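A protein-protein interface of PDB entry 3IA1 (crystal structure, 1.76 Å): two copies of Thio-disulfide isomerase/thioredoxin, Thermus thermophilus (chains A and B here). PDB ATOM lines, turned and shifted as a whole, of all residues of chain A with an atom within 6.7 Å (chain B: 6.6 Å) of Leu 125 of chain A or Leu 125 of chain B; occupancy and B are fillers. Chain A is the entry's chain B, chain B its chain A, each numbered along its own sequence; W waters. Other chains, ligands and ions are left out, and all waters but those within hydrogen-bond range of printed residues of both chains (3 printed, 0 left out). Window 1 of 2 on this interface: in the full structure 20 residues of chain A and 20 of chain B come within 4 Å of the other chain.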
ATOM      1  N   LYS A 106      -3.548  -6.294   5.743  1.00  0.00           N
ATOM      2  CA  LYS A 106      -2.919  -7.581   5.793  1.00  0.00           C
ATOM      3  C   LYS A 106      -3.290  -8.429   4.595  1.00  0.00           C
ATOM      4  O   LYS A 106      -3.389  -9.606   4.688  1.00  0.00           O
ATOM      5  CB  LYS A 106      -3.206  -8.275   7.114  1.00  0.00           C
ATOM      6  CG  LYS A 106      -2.372  -7.753   8.242  1.00  0.00           C
ATOM      7  CD  LYS A 106      -2.848  -8.190   9.574  1.00  0.00           C
ATOM      8  CE  LYS A 106      -3.459  -9.569   9.585  1.00  0.00           C
ATOM      9  NZ  LYS A 106      -3.647 -10.168  10.942  1.00  0.00           N
ATOM     10  N   VAL A 107      -3.460  -7.775   3.456  1.00  0.00           N
ATOM     11  CA  VAL A 107      -3.738  -8.457   2.224  1.00  0.00           C
ATOM     12  C   VAL A 107      -2.863  -7.977   1.072  1.00  0.00           C
ATOM     13  O   VAL A 107      -2.466  -6.861   1.041  1.00  0.00           O
ATOM     14  CB  VAL A 107      -5.201  -8.294   1.818  1.00  0.00           C
ATOM     15  CG1 VAL A 107      -6.093  -8.745   2.859  1.00  0.00           C
ATOM     16  CG2 VAL A 107      -5.475  -6.923   1.509  1.00  0.00           C
ATOM     17  N   TRP A 112      -9.771  -6.013  -3.560  1.00  0.00           N
ATOM     18  CA  TRP A 112     -10.285  -6.378  -2.248  1.00  0.00           C
ATOM     19  C   TRP A 112     -11.416  -5.437  -1.896  1.00  0.00           C
ATOM     20  O   TRP A 112     -11.361  -4.237  -2.199  1.00  0.00           O
ATOM     21  CB  TRP A 112      -9.191  -6.256  -1.168  1.00  0.00           C
ATOM     22  CG  TRP A 112      -8.163  -7.317  -1.261  1.00  0.00           C
ATOM     23  CD1 TRP A 112      -6.936  -7.234  -1.856  1.00  0.00           C
ATOM     24  CD2 TRP A 112      -8.258  -8.623  -0.715  1.00  0.00           C
ATOM     25  NE1 TRP A 112      -6.266  -8.428  -1.739  1.00  0.00           N
ATOM     26  CE2 TRP A 112      -7.063  -9.304  -1.046  1.00  0.00           C
ATOM     27  CE3 TRP A 112      -9.260  -9.301   0.007  1.00  0.00           C
ATOM     28  CZ2 TRP A 112      -6.823 -10.629  -0.661  1.00  0.00           C
ATOM     29  CZ3 TRP A 112      -9.020 -10.610   0.387  1.00  0.00           C
ATOM     30  CH2 TRP A 112      -7.815 -11.259   0.055  1.00  0.00           C
ATOM     31  N   THR A 113     -12.418  -5.976  -1.199  1.00  0.00           N
ATOM     32  CA  THR A 113     -13.538  -5.191  -0.666  1.00  0.00           C
ATOM     33  C   THR A 113     -13.599  -5.490   0.829  1.00  0.00           C
ATOM     34  O   THR A 113     -13.659  -6.641   1.212  1.00  0.00           O
ATOM     35  CB  THR A 113     -14.867  -5.610  -1.360  1.00  0.00           C
ATOM     36  OG1 THR A 113     -14.734  -5.391  -2.770  1.00  0.00           O
ATOM     37  CG2 THR A 113     -16.061  -4.803  -0.837  1.00  0.00           C
ATOM     38  N   PHE A 114     -13.550  -4.445   1.645  1.00  0.00           N
ATOM     39  CA  PHE A 114     -13.548  -4.552   3.121  1.00  0.00           C
ATOM     40  C   PHE A 114     -14.815  -3.889   3.657  1.00  0.00           C
ATOM     41  O   PHE A 114     -15.185  -2.780   3.239  1.00  0.00           O
ATOM     42  CB  PHE A 114     -12.367  -3.792   3.757  1.00  0.00           C
ATOM     43  CG  PHE A 114     -11.030  -4.142   3.199  1.00  0.00           C
ATOM     44  CD1 PHE A 114     -10.226  -5.105   3.821  1.00  0.00           C
ATOM     45  CD2 PHE A 114     -10.526  -3.459   2.096  1.00  0.00           C
ATOM     46  CE1 PHE A 114      -8.970  -5.403   3.321  1.00  0.00           C
ATOM     47  CE2 PHE A 114      -9.280  -3.773   1.578  1.00  0.00           C
ATOM     48  CZ  PHE A 114      -8.496  -4.739   2.192  1.00  0.00           C
ATOM     49  N   VAL A 115     -15.478  -4.547   4.600  1.00  0.00           N
ATOM     50  CA  VAL A 115     -16.635  -3.955   5.234  1.00  0.00           C
ATOM     51  C   VAL A 115     -16.221  -3.527   6.642  1.00  0.00           C
ATOM     52  O   VAL A 115     -15.691  -4.328   7.415  1.00  0.00           O
ATOM     53  CB  VAL A 115     -17.818  -4.960   5.293  1.00  0.00           C
ATOM     54  CG1 VAL A 115     -18.992  -4.385   6.056  1.00  0.00           C
ATOM     55  CG2 VAL A 115     -18.222  -5.349   3.865  1.00  0.00           C
ATOM     56  N   VAL A 122     -12.839  -4.092  10.625  1.00  0.00           N
ATOM     57  CA  VAL A 122     -13.055  -4.797   9.346  1.00  0.00           C
ATOM     58  C   VAL A 122     -13.647  -6.157   9.706  1.00  0.00           C
ATOM     59  O   VAL A 122     -12.941  -7.014  10.237  1.00  0.00           O
ATOM     60  CB  VAL A 122     -11.761  -4.956   8.550  1.00  0.00           C
ATOM     61  CG1 VAL A 122     -11.994  -5.809   7.297  1.00  0.00           C
ATOM     62  CG2 VAL A 122     -11.205  -3.563   8.167  1.00  0.00           C
ATOM     63  N   VAL A 123     -14.935  -6.338   9.420  1.00  0.00           N
ATOM     64  CA  VAL A 123     -15.704  -7.518   9.843  1.00  0.00           C
ATOM     65  C   VAL A 123     -16.035  -8.487   8.698  1.00  0.00           C
ATOM     66  O   VAL A 123     -16.601  -9.563   8.931  1.00  0.00           O
ATOM     67  CB  VAL A 123     -17.021  -7.121  10.554  1.00  0.00           C
ATOM     68  CG1 VAL A 123     -16.733  -6.491  11.943  1.00  0.00           C
ATOM     69  CG2 VAL A 123     -17.871  -6.145   9.687  1.00  0.00           C
ATOM     70  N   ALA A 124     -15.713  -8.085   7.465  1.00  0.00           N
ATOM     71  CA  ALA A 124     -15.835  -8.957   6.292  1.00  0.00           C
ATOM     72  C   ALA A 124     -14.903  -8.481   5.217  1.00  0.00           C
ATOM     73  O   ALA A 124     -14.698  -7.279   5.071  1.00  0.00           O
ATOM     74  CB  ALA A 124     -17.274  -8.976   5.761  1.00  0.00           C
ATOM     75  N   LEU A 125     -14.354  -9.431   4.461  1.00  0.00           N
ATOM     76  CA  LEU A 125     -13.542  -9.115   3.288  1.00  0.00           C
ATOM     77  C   LEU A 125     -13.957 -10.011   2.148  1.00  0.00           C
ATOM     78  O   LEU A 125     -14.412 -11.143   2.363  1.00  0.00           O
ATOM     79  CB  LEU A 125     -12.060  -9.359   3.534  1.00  0.00           C
ATOM     80  CG  LEU A 125     -11.276  -8.658   4.640  1.00  0.00           C
ATOM     81  CD1 LEU A 125     -11.447  -9.314   6.026  1.00  0.00           C
ATOM     82  CD2 LEU A 125      -9.812  -8.730   4.193  1.00  0.00           C
ATOM     83  N   PHE A 126     -13.767  -9.515   0.928  1.00  0.00           N
ATOM     84  CA  PHE A 126     -14.037 -10.300  -0.264  1.00  0.00           C
ATOM     85  C   PHE A 126     -12.908 -10.058  -1.233  1.00  0.00           C
ATOM     86  O   PHE A 126     -12.492  -8.910  -1.433  1.00  0.00           O
ATOM     87  CB  PHE A 126     -15.355  -9.823  -0.904  1.00  0.00           C
ATOM     88  CG  PHE A 126     -16.534  -9.912   0.024  1.00  0.00           C
ATOM     89  CD1 PHE A 126     -17.189 -11.134   0.206  1.00  0.00           C
ATOM     90  CD2 PHE A 126     -16.985  -8.779   0.727  1.00  0.00           C
ATOM     91  CE1 PHE A 126     -18.277 -11.232   1.062  1.00  0.00           C
ATOM     92  CE2 PHE A 126     -18.073  -8.858   1.587  1.00  0.00           C
ATOM     93  CZ  PHE A 126     -18.738 -10.097   1.751  1.00  0.00           C
ATOM     94  N   ALA A 127     -12.411 -11.150  -1.803  1.00  0.00           N
ATOM     95  CA  ALA A 127     -11.450 -11.123  -2.895  1.00  0.00           C
ATOM     96  C   ALA A 127     -12.194 -11.200  -4.222  1.00  0.00           C
ATOM     97  O   ALA A 127     -13.087 -12.013  -4.382  1.00  0.00           O
ATOM     98  CB  ALA A 127     -10.505 -12.300  -2.777  1.00  0.00           C
ATOM     99  N   ALA A 138     -23.213  -8.667   4.904  1.00  0.00           N
ATOM    100  CA  ALA A 138     -22.104  -8.133   5.701  1.00  0.00           C
ATOM    101  C   ALA A 138     -22.405  -6.706   6.172  1.00  0.00           C
ATOM    102  O   ALA A 138     -22.176  -6.379   7.329  1.00  0.00           O
ATOM    103  CB  ALA A 138     -20.789  -8.193   4.913  1.00  0.00           C
ATOM    104  N   PHE B 105      -2.180 -17.592  -0.425  1.00  0.00           N
ATOM    105  CA  PHE B 105      -3.550 -17.068  -0.301  1.00  0.00           C
ATOM    106  C   PHE B 105      -3.657 -15.535  -0.326  1.00  0.00           C
ATOM    107  O   PHE B 105      -4.750 -14.987  -0.174  1.00  0.00           O
ATOM    108  CB  PHE B 105      -4.211 -17.629   0.972  1.00  0.00           C
ATOM    109  CG  PHE B 105      -4.757 -19.031   0.792  1.00  0.00           C
ATOM    110  CD1 PHE B 105      -3.899 -20.127   0.651  1.00  0.00           C
ATOM    111  CD2 PHE B 105      -6.129 -19.244   0.777  1.00  0.00           C
ATOM    112  CE1 PHE B 105      -4.407 -21.424   0.509  1.00  0.00           C
ATOM    113  CE2 PHE B 105      -6.644 -20.553   0.638  1.00  0.00           C
ATOM    114  CZ  PHE B 105      -5.784 -21.625   0.499  1.00  0.00           C
ATOM    115  N   VAL B 107      -2.774 -13.294   1.832  1.00  0.00           N
ATOM    116  CA  VAL B 107      -3.089 -12.640   3.104  1.00  0.00           C
ATOM    117  C   VAL B 107      -1.915 -12.827   4.052  1.00  0.00           C
ATOM    118  O   VAL B 107      -1.131 -13.776   3.914  1.00  0.00           O
ATOM    119  CB  VAL B 107      -4.382 -13.175   3.786  1.00  0.00           C
ATOM    120  CG1 VAL B 107      -5.642 -12.941   2.911  1.00  0.00           C
ATOM    121  CG2 VAL B 107      -4.228 -14.643   4.204  1.00  0.00           C
ATOM    122  N   TRP B 112      -6.880 -16.309   9.961  1.00  0.00           N
ATOM    123  CA  TRP B 112      -7.802 -16.113   8.868  1.00  0.00           C
ATOM    124  C   TRP B 112      -8.793 -17.261   8.733  1.00  0.00           C
ATOM    125  O   TRP B 112      -8.500 -18.332   9.036  1.00  0.00           O
ATOM    126  CB  TRP B 112      -7.048 -15.953   7.551  1.00  0.00           C
ATOM    127  CG  TRP B 112      -6.323 -14.673   7.400  1.00  0.00           C
ATOM    128  CD1 TRP B 112      -5.039 -14.397   7.740  1.00  0.00           C
ATOM    129  CD2 TRP B 112      -6.833 -13.501   6.812  1.00  0.00           C
ATOM    130  NE1 TRP B 112      -4.734 -13.095   7.436  1.00  0.00           N
ATOM    131  CE2 TRP B 112      -5.829 -12.523   6.865  1.00  0.00           C
ATOM    132  CE3 TRP B 112      -8.049 -13.172   6.252  1.00  0.00           C
ATOM    133  CZ2 TRP B 112      -6.024 -11.265   6.379  1.00  0.00           C
ATOM    134  CZ3 TRP B 112      -8.229 -11.926   5.770  1.00  0.00           C
ATOM    135  CH2 TRP B 112      -7.230 -10.983   5.849  1.00  0.00           C
ATOM    136  N   THR B 113      -9.989 -16.921   8.281  1.00  0.00           N
ATOM    137  CA  THR B 113     -11.035 -17.905   7.989  1.00  0.00           C
ATOM    138  C   THR B 113     -11.504 -17.624   6.563  1.00  0.00           C
ATOM    139  O   THR B 113     -11.840 -16.475   6.255  1.00  0.00           O
ATOM    140  CB  THR B 113     -12.205 -17.708   8.966  1.00  0.00           C
ATOM    141  OG1 THR B 113     -11.725 -17.849  10.314  1.00  0.00           O
ATOM    142  CG2 THR B 113     -13.332 -18.699   8.703  1.00  0.00           C
ATOM    143  N   PHE B 114     -11.510 -18.665   5.722  1.00  0.00           N
ATOM    144  CA  PHE B 114     -11.879 -18.547   4.289  1.00  0.00           C
ATOM    145  C   PHE B 114     -13.075 -19.455   4.061  1.00  0.00           C
ATOM    146  O   PHE B 114     -13.028 -20.615   4.460  1.00  0.00           O
ATOM    147  CB  PHE B 114     -10.764 -19.065   3.366  1.00  0.00           C
ATOM    148  CG  PHE B 114      -9.415 -18.409   3.577  1.00  0.00           C
ATOM    149  CD1 PHE B 114      -9.010 -17.343   2.774  1.00  0.00           C
ATOM    150  CD2 PHE B 114      -8.533 -18.889   4.549  1.00  0.00           C
ATOM    151  CE1 PHE B 114      -7.739 -16.779   2.944  1.00  0.00           C
ATOM    152  CE2 PHE B 114      -7.277 -18.311   4.730  1.00  0.00           C
ATOM    153  CZ  PHE B 114      -6.891 -17.243   3.931  1.00  0.00           C
ATOM    154  N   VAL B 115     -14.103 -18.953   3.385  1.00  0.00           N
ATOM    155  CA  VAL B 115     -15.265 -19.788   3.018  1.00  0.00           C
ATOM    156  C   VAL B 115     -15.125 -20.139   1.528  1.00  0.00           C
ATOM    157  O   VAL B 115     -14.973 -19.249   0.685  1.00  0.00           O
ATOM    158  CB  VAL B 115     -16.588 -19.049   3.287  1.00  0.00           C
ATOM    159  CG1 VAL B 115     -17.767 -19.895   2.830  1.00  0.00           C
ATOM    160  CG2 VAL B 115     -16.733 -18.729   4.792  1.00  0.00           C
ATOM    161  N   VAL B 122     -13.099 -18.979  -3.162  1.00  0.00           N
ATOM    162  CA  VAL B 122     -13.139 -18.287  -1.874  1.00  0.00           C
ATOM    163  C   VAL B 122     -14.081 -17.091  -1.993  1.00  0.00           C
ATOM    164  O   VAL B 122     -13.761 -16.089  -2.651  1.00  0.00           O
ATOM    165  CB  VAL B 122     -11.720 -17.879  -1.396  1.00  0.00           C
ATOM    166  CG1 VAL B 122     -11.787 -17.092  -0.075  1.00  0.00           C
ATOM    167  CG2 VAL B 122     -10.832 -19.121  -1.252  1.00  0.00           C
ATOM    168  N   VAL B 123     -15.243 -17.207  -1.349  1.00  0.00           N
ATOM    169  CA  VAL B 123     -16.301 -16.213  -1.453  1.00  0.00           C
ATOM    170  C   VAL B 123     -16.514 -15.345  -0.220  1.00  0.00           C
ATOM    171  O   VAL B 123     -17.352 -14.436  -0.239  1.00  0.00           O
ATOM    172  CB  VAL B 123     -17.634 -16.909  -1.845  1.00  0.00           C
ATOM    173  CG1 VAL B 123     -17.512 -17.523  -3.235  1.00  0.00           C
ATOM    174  CG2 VAL B 123     -17.989 -17.995  -0.819  1.00  0.00           C
ATOM    175  N   ALA B 124     -15.785 -15.642   0.868  1.00  0.00           N
ATOM    176  CA  ALA B 124     -15.812 -14.793   2.057  1.00  0.00           C
ATOM    177  C   ALA B 124     -14.514 -15.001   2.819  1.00  0.00           C
ATOM    178  O   ALA B 124     -13.963 -16.107   2.836  1.00  0.00           O
ATOM    179  CB  ALA B 124     -17.034 -15.124   2.982  1.00  0.00           C
ATOM    180  N   LEU B 125     -14.008 -13.931   3.416  1.00  0.00           N
ATOM    181  CA  LEU B 125     -12.841 -14.027   4.271  1.00  0.00           C
ATOM    182  C   LEU B 125     -13.116 -13.240   5.540  1.00  0.00           C
ATOM    183  O   LEU B 125     -13.877 -12.255   5.538  1.00  0.00           O
ATOM    184  CB  LEU B 125     -11.576 -13.461   3.606  1.00  0.00           C
ATOM    185  CG  LEU B 125     -10.978 -14.077   2.335  1.00  0.00           C
ATOM    186  CD1 LEU B 125     -11.685 -13.518   1.081  1.00  0.00           C
ATOM    187  CD2 LEU B 125      -9.497 -13.781   2.298  1.00  0.00           C
ATOM    188  N   PHE B 126     -12.499 -13.679   6.637  1.00  0.00           N
ATOM    189  CA  PHE B 126     -12.588 -12.960   7.905  1.00  0.00           C
ATOM    190  C   PHE B 126     -11.205 -12.943   8.502  1.00  0.00           C
ATOM    191  O   PHE B 126     -10.535 -13.952   8.519  1.00  0.00           O
ATOM    192  CB  PHE B 126     -13.558 -13.683   8.868  1.00  0.00           C
ATOM    193  CG  PHE B 126     -14.938 -13.839   8.308  1.00  0.00           C
ATOM    194  CD1 PHE B 126     -15.823 -12.762   8.303  1.00  0.00           C
ATOM    195  CD2 PHE B 126     -15.320 -15.034   7.702  1.00  0.00           C
ATOM    196  CE1 PHE B 126     -17.110 -12.911   7.745  1.00  0.00           C
ATOM    197  CE2 PHE B 126     -16.603 -15.192   7.143  1.00  0.00           C
ATOM    198  CZ  PHE B 126     -17.485 -14.134   7.159  1.00  0.00           C
ATOM    199  N   ALA B 127     -10.780 -11.769   8.954  1.00  0.00           N
ATOM    200  CA  ALA B 127      -9.493 -11.600   9.598  1.00  0.00           C
ATOM    201  C   ALA B 127      -9.758 -11.541  11.095  1.00  0.00           C
ATOM    202  O   ALA B 127     -10.698 -10.894  11.524  1.00  0.00           O
ATOM    203  CB  ALA B 127      -8.805 -10.302   9.099  1.00  0.00           C
HETATM  204  O   HOH W   1     -14.083 -13.458  -1.577  1.00  0.00           O
HETATM  205  O   HOH W   2     -16.645 -11.969   4.246  1.00  0.00           O
HETATM  206  O   HOH W   3     -12.831  -9.732   9.307  1.00  0.00           O
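Water W1 bridges N of Ala 127 of chain A (2.9 Å) and O of Val 122 of chain B (2.9 Å). Water W3 lies within hydrogen-bond range of O of Val 122 of chain A and N of Ala 127 of chain B. Water W2 lies within hydrogen-bond range of the backbone carbonyl oxygen (O) of Leu 125 of chain A and the backbone carbonyl oxygen (O) of Leu 125 of chain B.
Of the printed residues of chain B, Lys 106 of chain A touches Val 107 and Trp 112. Printed residues of chain B within 4 Å of Val 123 of chain A: Phe 126. Leu 125 of chain A touches just these residues of chain B: Trp 112 (3.8 Å), Ala 124 (3.9 Å), Leu 125 (3.0 Å) and Ala 127 (3.9 Å). Printed residues of chain A within 4 Å of Val 107 of chain B: Lys 106 (3.4 Å) and Trp 112 (3.96 Å). Of chain A, only Trp 112 (3.7 Å), Ala 124 (3.9 Å), Leu 125 (3.0 Å) and Ala 127 (3.8 Å) come within 4 Å of Leu 125 of chain B. The nearest residue of chain A that does not touch Leu 125 of chain B is Phe 126 of chain A (4.2 Å). The nearest printed residue of chain B that does not touch Ala 127 of chain A is Val 122 of chain B (4.5 Å).
O of Thr 113 of chain B lies within hydrogen-bond range of N of Phe 126 of chain B, at 2.9 Å. The backbone carbonyl oxygen (O) of Val 115 of chain B lies within hydrogen-bond range of the backbone NH (N) of Val 123 of chain B, 2.9 Å away. The backbone NH (N) of Val 115 of chain B sits at hydrogen-bond distance from the backbone carbonyl oxygen (O) of Ala 124 of chain B (2.9 Å). The backbone carbonyl oxygen (O) of Thr 113 of chain A sits at hydrogen-bond distance from the backbone NH (N) of Phe 126 of chain A, 2.9 Å away. N of Val 123 of chain A is in hydrogen-bond range of O of Val 115 of chain A (2.9 Å). N of Val 115 of chain A sits at hydrogen-bond distance from O of Ala 124 of chain A (2.9 Å).
Among the printed residues, pairs that only touch across the chains: Phe 126 of chain A with Val 123 of chain B (3.3 Å), Val 123 of chain A with Phe 126 of chain B (3.4 Å), Lys 106 of chain A with Val 107 of chain B (3.4 Å), Lys 106 of chain A with Trp 112 of chain B (3.5 Å), Trp 112 of chain A with Leu 125 of chain B (3.7 Å), Ala 127 of chain A with Leu 125 of chain B (3.8 Å), Leu 125 of chain A with Trp 112 of chain B (3.8 Å), Leu 125 of chain A with Ala 127 of chain B (3.9 Å), Leu 125 of chain A with Ala 124 of chain B (3.9 Å), Val 107 of chain A with Trp 112 of chain B (3.9 Å), Ala 124 of chain A with Leu 125 of chain B (3.9 Å) and Trp 112 of chain A with Val 107 of chain B (3.96 Å).
Val 107 of chain A touches Trp 112 of chain B, and with the chains exchanged Trp 112 of chain A touches Val 107 of chain B. Val 123 of chain A touches Phe 126 of chain B, and with the chains exchanged Phe 126 of chain A touches Val 123 of chain B. Ala 124 of chain A touches Leu 125 of chain B, and with the chains exchanged Leu 125 of chain A touches Ala 124 of chain B. Leu 125 of chain A touches Ala 127 of chain B, and with the chains exchanged Ala 127 of chain A touches Leu 125 of chain B. Positions printed for both chains: 107, 112, 113, 114, 115, 122, 123, 124, 125, 126 and 127.
The backbone carbonyl oxygen (O) of Leu 125 of chain A lies within hydrogen-bond range of the backbone NH (N) of Leu 125 of chain B (3.0 Å).
Of the 13 printed residues of chain A, 8 touch a printed residue of chain B. Printed residues of chain A that touch a printed residue of chain B: Lys 106, Val 107, Trp 112, Val 123, Ala 124, Leu 125, Phe 126 and Ala 127. Hydrophobic or aromatic side chains of chain A within 4 Å of the printed part of chain B: Val 107, Trp 112, Leu 125 and Phe 126. Among the printed residues, 13 pairs touch across the chains. Among the printed residues, no Asp or Glu carboxylate lies within 4 Å of a Lys or Arg side-chain nitrogen of the other chain.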
